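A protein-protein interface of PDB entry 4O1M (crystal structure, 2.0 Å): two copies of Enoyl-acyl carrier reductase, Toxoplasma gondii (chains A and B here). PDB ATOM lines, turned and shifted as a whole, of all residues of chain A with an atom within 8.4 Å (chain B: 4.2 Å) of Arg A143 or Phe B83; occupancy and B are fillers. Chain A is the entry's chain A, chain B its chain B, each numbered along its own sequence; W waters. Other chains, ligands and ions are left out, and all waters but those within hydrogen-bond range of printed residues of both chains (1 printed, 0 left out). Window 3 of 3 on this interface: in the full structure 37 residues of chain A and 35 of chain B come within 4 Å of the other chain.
OH of Tyr B155 touches C of Ser A142, at 3.4 Å.
N of Phe B83 touches NH2 of Arg A143 (3.9 Å).
CD1 of Ile B107 touches NH2 of Arg A143, 3.9 Å away.
Tyr B155 touches Tyr A146.
Ser B151 touches Leu A147 (N to CD2, 3.9 Å).
Of the 14 printed residues of chain A, 5 touch a printed residue of chain B.
Hydrophobic or aromatic side chains of chain A that line the printed part of chain B: Tyr A146 and Leu A147.
Along chain A the printed residues that touch a printed residue of chain B span positions 141 to 147.
Of the 14 printed residues of chain B, 7 touch a printed residue of chain A.
Among the printed residues, 11 pairs touch across the chains.
OE2 of Glu A133 lies within hydrogen-bond range of OG of Ser A142, 2.6 Å away.
The side-chain hydroxyl of Thr A141 lies close to the backbone NH of Gly A191 (3.4 Å).
The backbone NH (N) of Gly A145 sits at hydrogen-bond distance from the side-chain hydroxyl (OG) of Ser A142, at 2.9 Å.
OD1 of Asp B80 sits at hydrogen-bond distance from N of Ala B82, 3.1 Å away.
The backbone carbonyl oxygen (O) of Phe B83 lies within hydrogen-bond range of the backbone NH (N) of Ile B107 (3.0 Å).
OD2 of Asp B88 lies within hydrogen-bond range of N of Asp B84, at 3.2 Å.
Arg A143 touches just these residues of chain B: Ala B81, Ala B82, Phe B83, Asp B84, Ile B107, Ser B151 and Tyr B155.
Phe B83 touches just one residue of chain A: Arg A143.
Of chain A, only Arg A143 (3.3 Å) comes within 4 Å of Ala B82.
Of the printed residues of chain B, Ser A142 touches Tyr B155 (3.4 Å).
Printed residues of chain B within 4 Å of Thr A141: Tyr B155.
Of the printed residues of chain B, Leu A147 touches Ser B151.
Asp B88 touches none of the printed residues of chain A.
Val B89 touches none of the printed residues of chain A.
The nearest printed residue of chain A that does not touch Phe B83 is Leu A147 (9.3 Å).
The nearest printed residue of chain A that does not touch Ile B107 is Thr A141 (10.3 Å).
The backbone carbonyl oxygen (O) of Thr A141 is in hydrogen-bond range of the side-chain hydroxyl (OH) of Tyr B155, at 2.7 Å.
NH2 of Arg A143 sits at hydrogen-bond distance from O of Ala B81 (2.8 Å).
NE of Arg A143 sits close to O of Ala B82 (3.4 Å).
OD1 of Asp B84 lies within salt-bridge range of NH2 of Arg A143.
OG of Ser B151 lies within hydrogen-bond range of NH1 of Arg A143, 2.7 Å away.
The side-chain hydroxyl of Tyr B155 lies within hydrogen-bond range of the backbone NH of Arg A143.
Water W1 lies within hydrogen-bond range of the side-chain carboxylate (OD2) of Asp B84 (2.8 Å), the backbone NH (N) of Arg A143 (2.9 Å) and the side-chain hydroxyl (OH) of Tyr B155 (3.5 Å).
No position is printed for both chains.
Of the 11 pairs that touch across the chains among the printed residues, none has its exchanged pair printed and touching as well.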
ATOM      1  N   GLU A 133      16.108 -20.990  20.253  1.00  0.00           N
ATOM      2  CA  GLU A 133      14.937 -20.304  19.695  1.00  0.00           C
ATOM      3  C   GLU A 133      14.891 -18.812  20.056  1.00  0.00           C
ATOM      4  O   GLU A 133      13.809 -18.195  20.148  1.00  0.00           O
ATOM      5  CB  GLU A 133      13.642 -21.019  20.135  1.00  0.00           C
ATOM      6  CG  GLU A 133      13.563 -22.495  19.602  1.00  0.00           C
ATOM      7  CD  GLU A 133      12.222 -23.204  19.896  1.00  0.00           C
ATOM      8  OE1 GLU A 133      11.296 -22.549  20.404  1.00  0.00           O
ATOM      9  OE2 GLU A 133      12.093 -24.427  19.618  1.00  0.00           O
ATOM     10  N   LEU A 138       8.149 -15.394  23.066  1.00  0.00           N
ATOM     11  CA  LEU A 138       7.808 -16.426  24.051  1.00  0.00           C
ATOM     12  C   LEU A 138       6.514 -17.196  23.703  1.00  0.00           C
ATOM     13  O   LEU A 138       6.441 -18.423  23.895  1.00  0.00           O
ATOM     14  CB  LEU A 138       7.733 -15.800  25.437  1.00  0.00           C
ATOM     15  CG  LEU A 138       7.958 -16.664  26.670  1.00  0.00           C
ATOM     16  CD1 LEU A 138       9.231 -17.552  26.573  1.00  0.00           C
ATOM     17  CD2 LEU A 138       8.019 -15.752  27.887  1.00  0.00           C
ATOM     18  N   GLU A 140       5.780 -18.172  20.897  1.00  0.00           N
ATOM     19  CA  GLU A 140       6.086 -19.115  19.796  1.00  0.00           C
ATOM     20  C   GLU A 140       7.289 -20.014  20.157  1.00  0.00           C
ATOM     21  O   GLU A 140       7.856 -20.657  19.301  1.00  0.00           O
ATOM     22  CB  GLU A 140       6.402 -18.339  18.509  1.00  0.00           C
ATOM     23  CG  GLU A 140       5.198 -17.606  17.917  1.00  0.00           C
ATOM     24  CD  GLU A 140       5.612 -16.506  16.917  1.00  0.00           C
ATOM     25  OE1 GLU A 140       6.638 -16.652  16.203  1.00  0.00           O
ATOM     26  OE2 GLU A 140       4.900 -15.484  16.838  1.00  0.00           O
ATOM     27  N   THR A 141       7.704 -19.993  21.415  1.00  0.00           N
ATOM     28  CA  THR A 141       8.845 -20.790  21.879  1.00  0.00           C
ATOM     29  C   THR A 141       8.374 -22.167  22.376  1.00  0.00           C
ATOM     30  O   THR A 141       7.452 -22.251  23.216  1.00  0.00           O
ATOM     31  CB  THR A 141       9.573 -20.032  23.002  1.00  0.00           C
ATOM     32  OG1 THR A 141      10.174 -18.855  22.454  1.00  0.00           O
ATOM     33  CG2 THR A 141      10.695 -20.886  23.647  1.00  0.00           C
ATOM     34  N   SER A 142       8.994 -23.239  21.867  1.00  0.00           N
ATOM     35  CA  SER A 142       8.644 -24.629  22.262  1.00  0.00           C
ATOM     36  C   SER A 142       9.262 -24.963  23.655  1.00  0.00           C
ATOM     37  O   SER A 142      10.230 -24.302  24.108  1.00  0.00           O
ATOM     38  CB  SER A 142       9.198 -25.637  21.229  1.00  0.00           C
ATOM     39  OG  SER A 142      10.641 -25.720  21.379  1.00  0.00           O
ATOM     40  N   ARG A 143       8.728 -26.015  24.296  1.00  0.00           N
ATOM     41  CA  ARG A 143       9.236 -26.455  25.597  1.00  0.00           C
ATOM     42  C   ARG A 143      10.687 -26.858  25.438  1.00  0.00           C
ATOM     43  O   ARG A 143      11.530 -26.493  26.235  1.00  0.00           O
ATOM     44  CB  ARG A 143       8.407 -27.645  26.144  1.00  0.00           C
ATOM     45  CG  ARG A 143       8.780 -28.071  27.600  1.00  0.00           C
ATOM     46  CD  ARG A 143       7.825 -29.263  28.027  1.00  0.00           C
ATOM     47  NE  ARG A 143       6.443 -28.795  28.138  1.00  0.00           N
ATOM     48  CZ  ARG A 143       5.802 -28.442  29.259  1.00  0.00           C
ATOM     49  NH1 ARG A 143       6.402 -28.436  30.452  1.00  0.00           N
ATOM     50  NH2 ARG A 143       4.526 -28.070  29.177  1.00  0.00           N
ATOM     51  N   LYS A 144      10.981 -27.586  24.370  1.00  0.00           N
ATOM     52  CA  LYS A 144      12.337 -28.033  24.118  1.00  0.00           C
ATOM     53  C   LYS A 144      13.301 -26.844  23.949  1.00  0.00           C
ATOM     54  O   LYS A 144      14.397 -26.858  24.496  1.00  0.00           O
ATOM     55  CB  LYS A 144      12.336 -28.971  22.916  1.00  0.00           C
ATOM     56  CG  LYS A 144      13.695 -29.508  22.489  1.00  0.00           C
ATOM     57  CD  LYS A 144      13.450 -30.549  21.368  1.00  0.00           C
ATOM     58  CE  LYS A 144      14.708 -30.868  20.557  1.00  0.00           C
ATOM     59  NZ  LYS A 144      15.815 -31.287  21.452  1.00  0.00           N
ATOM     60  N   GLY A 145      12.895 -25.800  23.232  1.00  0.00           N
ATOM     61  CA  GLY A 145      13.779 -24.640  23.048  1.00  0.00           C
ATOM     62  C   GLY A 145      13.989 -23.891  24.356  1.00  0.00           C
ATOM     63  O   GLY A 145      15.101 -23.429  24.682  1.00  0.00           O
ATOM     64  N   TYR A 146      12.918 -23.768  25.125  1.00  0.00           N
ATOM     65  CA  TYR A 146      12.971 -23.046  26.367  1.00  0.00           C
ATOM     66  C   TYR A 146      13.910 -23.754  27.363  1.00  0.00           C
ATOM     67  O   TYR A 146      14.726 -23.110  28.056  1.00  0.00           O
ATOM     68  CB  TYR A 146      11.556 -22.977  26.913  1.00  0.00           C
ATOM     69  CG  TYR A 146      11.367 -22.232  28.203  1.00  0.00           C
ATOM     70  CD1 TYR A 146      11.527 -22.884  29.425  1.00  0.00           C
ATOM     71  CD2 TYR A 146      10.880 -20.915  28.191  1.00  0.00           C
ATOM     72  CE1 TYR A 146      11.291 -22.227  30.636  1.00  0.00           C
ATOM     73  CE2 TYR A 146      10.637 -20.213  29.403  1.00  0.00           C
ATOM     74  CZ  TYR A 146      10.855 -20.894  30.618  1.00  0.00           C
ATOM     75  OH  TYR A 146      10.599 -20.282  31.819  1.00  0.00           O
ATOM     76  N   LEU A 147      13.769 -25.069  27.428  1.00  0.00           N
ATOM     77  CA  LEU A 147      14.542 -25.855  28.375  1.00  0.00           C
ATOM     78  C   LEU A 147      16.004 -25.927  27.945  1.00  0.00           C
ATOM     79  O   LEU A 147      16.862 -25.972  28.792  1.00  0.00           O
ATOM     80  CB  LEU A 147      13.937 -27.278  28.543  1.00  0.00           C
ATOM     81  CG  LEU A 147      12.589 -27.326  29.322  1.00  0.00           C
ATOM     82  CD1 LEU A 147      11.962 -28.789  29.313  1.00  0.00           C
ATOM     83  CD2 LEU A 147      12.691 -26.722  30.714  1.00  0.00           C
ATOM     84  N   ALA A 148      16.268 -25.973  26.635  1.00  0.00           N
ATOM     85  CA  ALA A 148      17.651 -25.900  26.130  1.00  0.00           C
ATOM     86  C   ALA A 148      18.276 -24.562  26.517  1.00  0.00           C
ATOM     87  O   ALA A 148      19.445 -24.526  26.969  1.00  0.00           O
ATOM     88  CB  ALA A 148      17.722 -26.109  24.614  1.00  0.00           C
ATOM     89  N   ALA A 149      17.517 -23.465  26.379  1.00  0.00           N
ATOM     90  CA  ALA A 149      18.049 -22.169  26.816  1.00  0.00           C
ATOM     91  C   ALA A 149      18.475 -22.236  28.289  1.00  0.00           C
ATOM     92  O   ALA A 149      19.544 -21.731  28.666  1.00  0.00           O
ATOM     93  CB  ALA A 149      17.026 -21.058  26.602  1.00  0.00           C
ATOM     94  N   SER A 150      17.605 -22.812  29.122  1.00  0.00           N
ATOM     95  CA  SER A 150      17.835 -22.854  30.574  1.00  0.00           C
ATOM     96  C   SER A 150      19.003 -23.819  30.879  1.00  0.00           C
ATOM     97  O   SER A 150      19.908 -23.501  31.676  1.00  0.00           O
ATOM     98  CB  SER A 150      16.560 -23.329  31.291  1.00  0.00           C
ATOM     99  OG  SER A 150      16.840 -23.637  32.630  1.00  0.00           O
ATOM    100  N   GLY A 191      12.905 -16.886  22.905  1.00  0.00           N
ATOM    101  CA  GLY A 191      13.265 -18.278  23.089  1.00  0.00           C
ATOM    102  C   GLY A 191      13.464 -18.709  24.520  1.00  0.00           C
ATOM    103  O   GLY A 191      14.098 -19.740  24.776  1.00  0.00           O
ATOM    104  N   ASP B  80      -2.164 -32.626  32.471  1.00  0.00           N
ATOM    105  CA  ASP B  80      -0.774 -32.748  32.884  1.00  0.00           C
ATOM    106  C   ASP B  80       0.053 -31.681  32.191  1.00  0.00           C
ATOM    107  O   ASP B  80       0.367 -31.777  30.992  1.00  0.00           O
ATOM    108  CB  ASP B  80      -0.219 -34.161  32.618  1.00  0.00           C
ATOM    109  CG  ASP B  80       1.113 -34.397  33.324  1.00  0.00           C
ATOM    110  OD1 ASP B  80       1.858 -33.427  33.521  1.00  0.00           O
ATOM    111  OD2 ASP B  80       1.411 -35.536  33.755  1.00  0.00           O
ATOM    112  N   ALA B  81       0.432 -30.654  32.953  1.00  0.00           N
ATOM    113  CA  ALA B  81       1.055 -29.496  32.386  1.00  0.00           C
ATOM    114  C   ALA B  81       2.549 -29.710  32.027  1.00  0.00           C
ATOM    115  O   ALA B  81       3.212 -28.768  31.600  1.00  0.00           O
ATOM    116  CB  ALA B  81       0.897 -28.313  33.365  1.00  0.00           C
ATOM    117  N   ALA B  82       3.073 -30.923  32.233  1.00  0.00           N
ATOM    118  CA  ALA B  82       4.399 -31.272  31.723  1.00  0.00           C
ATOM    119  C   ALA B  82       4.345 -31.565  30.198  1.00  0.00           C
ATOM    120  O   ALA B  82       5.379 -31.691  29.547  1.00  0.00           O
ATOM    121  CB  ALA B  82       4.953 -32.509  32.470  1.00  0.00           C
ATOM    122  N   PHE B  83       3.150 -31.696  29.626  1.00  0.00           N
ATOM    123  CA  PHE B  83       3.039 -32.143  28.223  1.00  0.00           C
ATOM    124  C   PHE B  83       2.199 -31.162  27.423  1.00  0.00           C
ATOM    125  O   PHE B  83       1.064 -30.867  27.804  1.00  0.00           O
ATOM    126  CB  PHE B  83       2.395 -33.535  28.192  1.00  0.00           C
ATOM    127  CG  PHE B  83       3.136 -34.544  29.023  1.00  0.00           C
ATOM    128  CD1 PHE B  83       4.485 -34.779  28.793  1.00  0.00           C
ATOM    129  CD2 PHE B  83       2.494 -35.243  30.041  1.00  0.00           C
ATOM    130  CE1 PHE B  83       5.180 -35.702  29.573  1.00  0.00           C
ATOM    131  CE2 PHE B  83       3.185 -36.186  30.812  1.00  0.00           C
ATOM    132  CZ  PHE B  83       4.515 -36.408  30.590  1.00  0.00           C
ATOM    133  N   ASP B  84       2.737 -30.673  26.316  1.00  0.00           N
ATOM    134  CA  ASP B  84       2.004 -29.711  25.484  1.00  0.00           C
ATOM    135  C   ASP B  84       1.087 -30.359  24.460  1.00  0.00           C
ATOM    136  O   ASP B  84       0.011 -29.818  24.180  1.00  0.00           O
ATOM    137  CB  ASP B  84       2.974 -28.769  24.782  1.00  0.00           C
ATOM    138  CG  ASP B  84       3.869 -28.071  25.769  1.00  0.00           C
ATOM    139  OD1 ASP B  84       3.336 -27.420  26.695  1.00  0.00           O
ATOM    140  OD2 ASP B  84       5.096 -28.240  25.676  1.00  0.00           O
ATOM    141  N   LYS B  85       1.512 -31.503  23.924  1.00  0.00           N
ATOM    142  CA  LYS B  85       0.804 -32.191  22.834  1.00  0.00           C
ATOM    143  C   LYS B  85       0.947 -33.690  23.017  1.00  0.00           C
ATOM    144  O   LYS B  85       1.881 -34.129  23.668  1.00  0.00           O
ATOM    145  CB  LYS B  85       1.460 -31.855  21.486  1.00  0.00           C
ATOM    146  CG  LYS B  85       1.470 -30.397  21.092  1.00  0.00           C
ATOM    147  CD  LYS B  85       2.313 -30.164  19.839  1.00  0.00           C
ATOM    148  CE  LYS B  85       3.727 -30.720  19.976  1.00  0.00           C
ATOM    149  NZ  LYS B  85       4.599 -29.896  20.851  1.00  0.00           N
ATOM    150  N   ASP B  88       4.290 -35.576  22.858  1.00  0.00           N
ATOM    151  CA  ASP B  88       5.244 -35.383  23.980  1.00  0.00           C
ATOM    152  C   ASP B  88       5.141 -36.458  25.078  1.00  0.00           C
ATOM    153  O   ASP B  88       6.030 -36.584  25.921  1.00  0.00           O
ATOM    154  CB  ASP B  88       5.054 -34.016  24.657  1.00  0.00           C
ATOM    155  CG  ASP B  88       5.207 -32.847  23.685  1.00  0.00           C
ATOM    156  OD1 ASP B  88       6.041 -32.942  22.767  1.00  0.00           O
ATOM    157  OD2 ASP B  88       4.450 -31.850  23.822  1.00  0.00           O
ATOM    158  N   VAL B  89       4.033 -37.186  25.124  1.00  0.00           N
ATOM    159  CA  VAL B  89       3.795 -38.077  26.245  1.00  0.00           C
ATOM    160  C   VAL B  89       4.549 -39.391  26.036  1.00  0.00           C
ATOM    161  O   VAL B  89       4.258 -40.108  25.088  1.00  0.00           O
ATOM    162  CB  VAL B  89       2.285 -38.371  26.398  1.00  0.00           C
ATOM    163  CG1 VAL B  89       2.032 -39.252  27.648  1.00  0.00           C
ATOM    164  CG2 VAL B  89       1.497 -37.066  26.479  1.00  0.00           C
ATOM    165  N   PRO B  90       5.516 -39.722  26.914  1.00  0.00           N
ATOM    166  CA  PRO B  90       6.232 -41.002  26.745  1.00  0.00           C
ATOM    167  C   PRO B  90       5.355 -42.214  26.946  1.00  0.00           C
ATOM    168  O   PRO B  90       4.340 -42.144  27.634  1.00  0.00           O
ATOM    169  CB  PRO B  90       7.322 -40.977  27.809  1.00  0.00           C
ATOM    170  CG  PRO B  90       7.088 -39.741  28.641  1.00  0.00           C
ATOM    171  CD  PRO B  90       5.922 -38.980  28.120  1.00  0.00           C
ATOM    172  N   ILE B  93       4.336 -43.260  30.582  1.00  0.00           N
ATOM    173  CA  ILE B  93       3.237 -42.480  31.163  1.00  0.00           C
ATOM    174  C   ILE B  93       1.899 -42.982  30.619  1.00  0.00           C
ATOM    175  O   ILE B  93       0.985 -43.248  31.392  1.00  0.00           O
ATOM    176  CB  ILE B  93       3.383 -40.932  30.930  1.00  0.00           C
ATOM    177  CG1 ILE B  93       4.595 -40.346  31.680  1.00  0.00           C
ATOM    178  CG2 ILE B  93       2.091 -40.194  31.295  1.00  0.00           C
ATOM    179  CD1 ILE B  93       4.583 -40.546  33.200  1.00  0.00           C
ATOM    180  N   THR B 106      -3.098 -33.423  27.588  1.00  0.00           N
ATOM    181  CA  THR B 106      -2.021 -32.458  27.311  1.00  0.00           C
ATOM    182  C   THR B 106      -2.638 -31.049  27.221  1.00  0.00           C
ATOM    183  O   THR B 106      -3.861 -30.895  27.017  1.00  0.00           O
ATOM    184  CB  THR B 106      -1.223 -32.763  26.048  1.00  0.00           C
ATOM    185  OG1 THR B 106      -2.090 -32.626  24.903  1.00  0.00           O
ATOM    186  CG2 THR B 106      -0.621 -34.181  26.127  1.00  0.00           C
ATOM    187  N   ILE B 107      -1.810 -30.031  27.439  1.00  0.00           N
ATOM    188  CA  ILE B 107      -2.308 -28.654  27.469  1.00  0.00           C
ATOM    189  C   ILE B 107      -3.082 -28.274  26.191  1.00  0.00           C
ATOM    190  O   ILE B 107      -4.196 -27.733  26.254  1.00  0.00           O
ATOM    191  CB  ILE B 107      -1.154 -27.669  27.733  1.00  0.00           C
ATOM    192  CG1 ILE B 107      -0.523 -27.969  29.102  1.00  0.00           C
ATOM    193  CG2 ILE B 107      -1.648 -26.214  27.580  1.00  0.00           C
ATOM    194  CD1 ILE B 107       0.765 -27.120  29.425  1.00  0.00           C
ATOM    195  N   SER B 151      10.327 -27.015  33.749  1.00  0.00           N
ATOM    196  CA  SER B 151       9.293 -27.517  32.861  1.00  0.00           C
ATOM    197  C   SER B 151       7.904 -27.512  33.499  1.00  0.00           C
ATOM    198  O   SER B 151       6.930 -27.049  32.913  1.00  0.00           O
ATOM    199  CB  SER B 151       9.631 -28.942  32.453  1.00  0.00           C
ATOM    200  OG  SER B 151       8.758 -29.345  31.413  1.00  0.00           O
ATOM    201  N   TYR B 155       7.665 -23.142  32.487  1.00  0.00           N
ATOM    202  CA  TYR B 155       7.196 -23.297  31.097  1.00  0.00           C
ATOM    203  C   TYR B 155       5.690 -23.663  30.996  1.00  0.00           C
ATOM    204  O   TYR B 155       5.020 -23.237  30.053  1.00  0.00           O
ATOM    205  CB  TYR B 155       8.048 -24.255  30.263  1.00  0.00           C
ATOM    206  CG  TYR B 155       7.606 -24.223  28.803  1.00  0.00           C
ATOM    207  CD1 TYR B 155       8.043 -23.210  27.937  1.00  0.00           C
ATOM    208  CD2 TYR B 155       6.676 -25.136  28.329  1.00  0.00           C
ATOM    209  CE1 TYR B 155       7.606 -23.137  26.625  1.00  0.00           C
ATOM    210  CE2 TYR B 155       6.219 -25.063  27.041  1.00  0.00           C
ATOM    211  CZ  TYR B 155       6.694 -24.069  26.178  1.00  0.00           C
ATOM    212  OH  TYR B 155       6.235 -24.038  24.867  1.00  0.00           O
HETATM  213  O   HOH W   1       6.295 -27.154  23.344  1.00  0.00           O
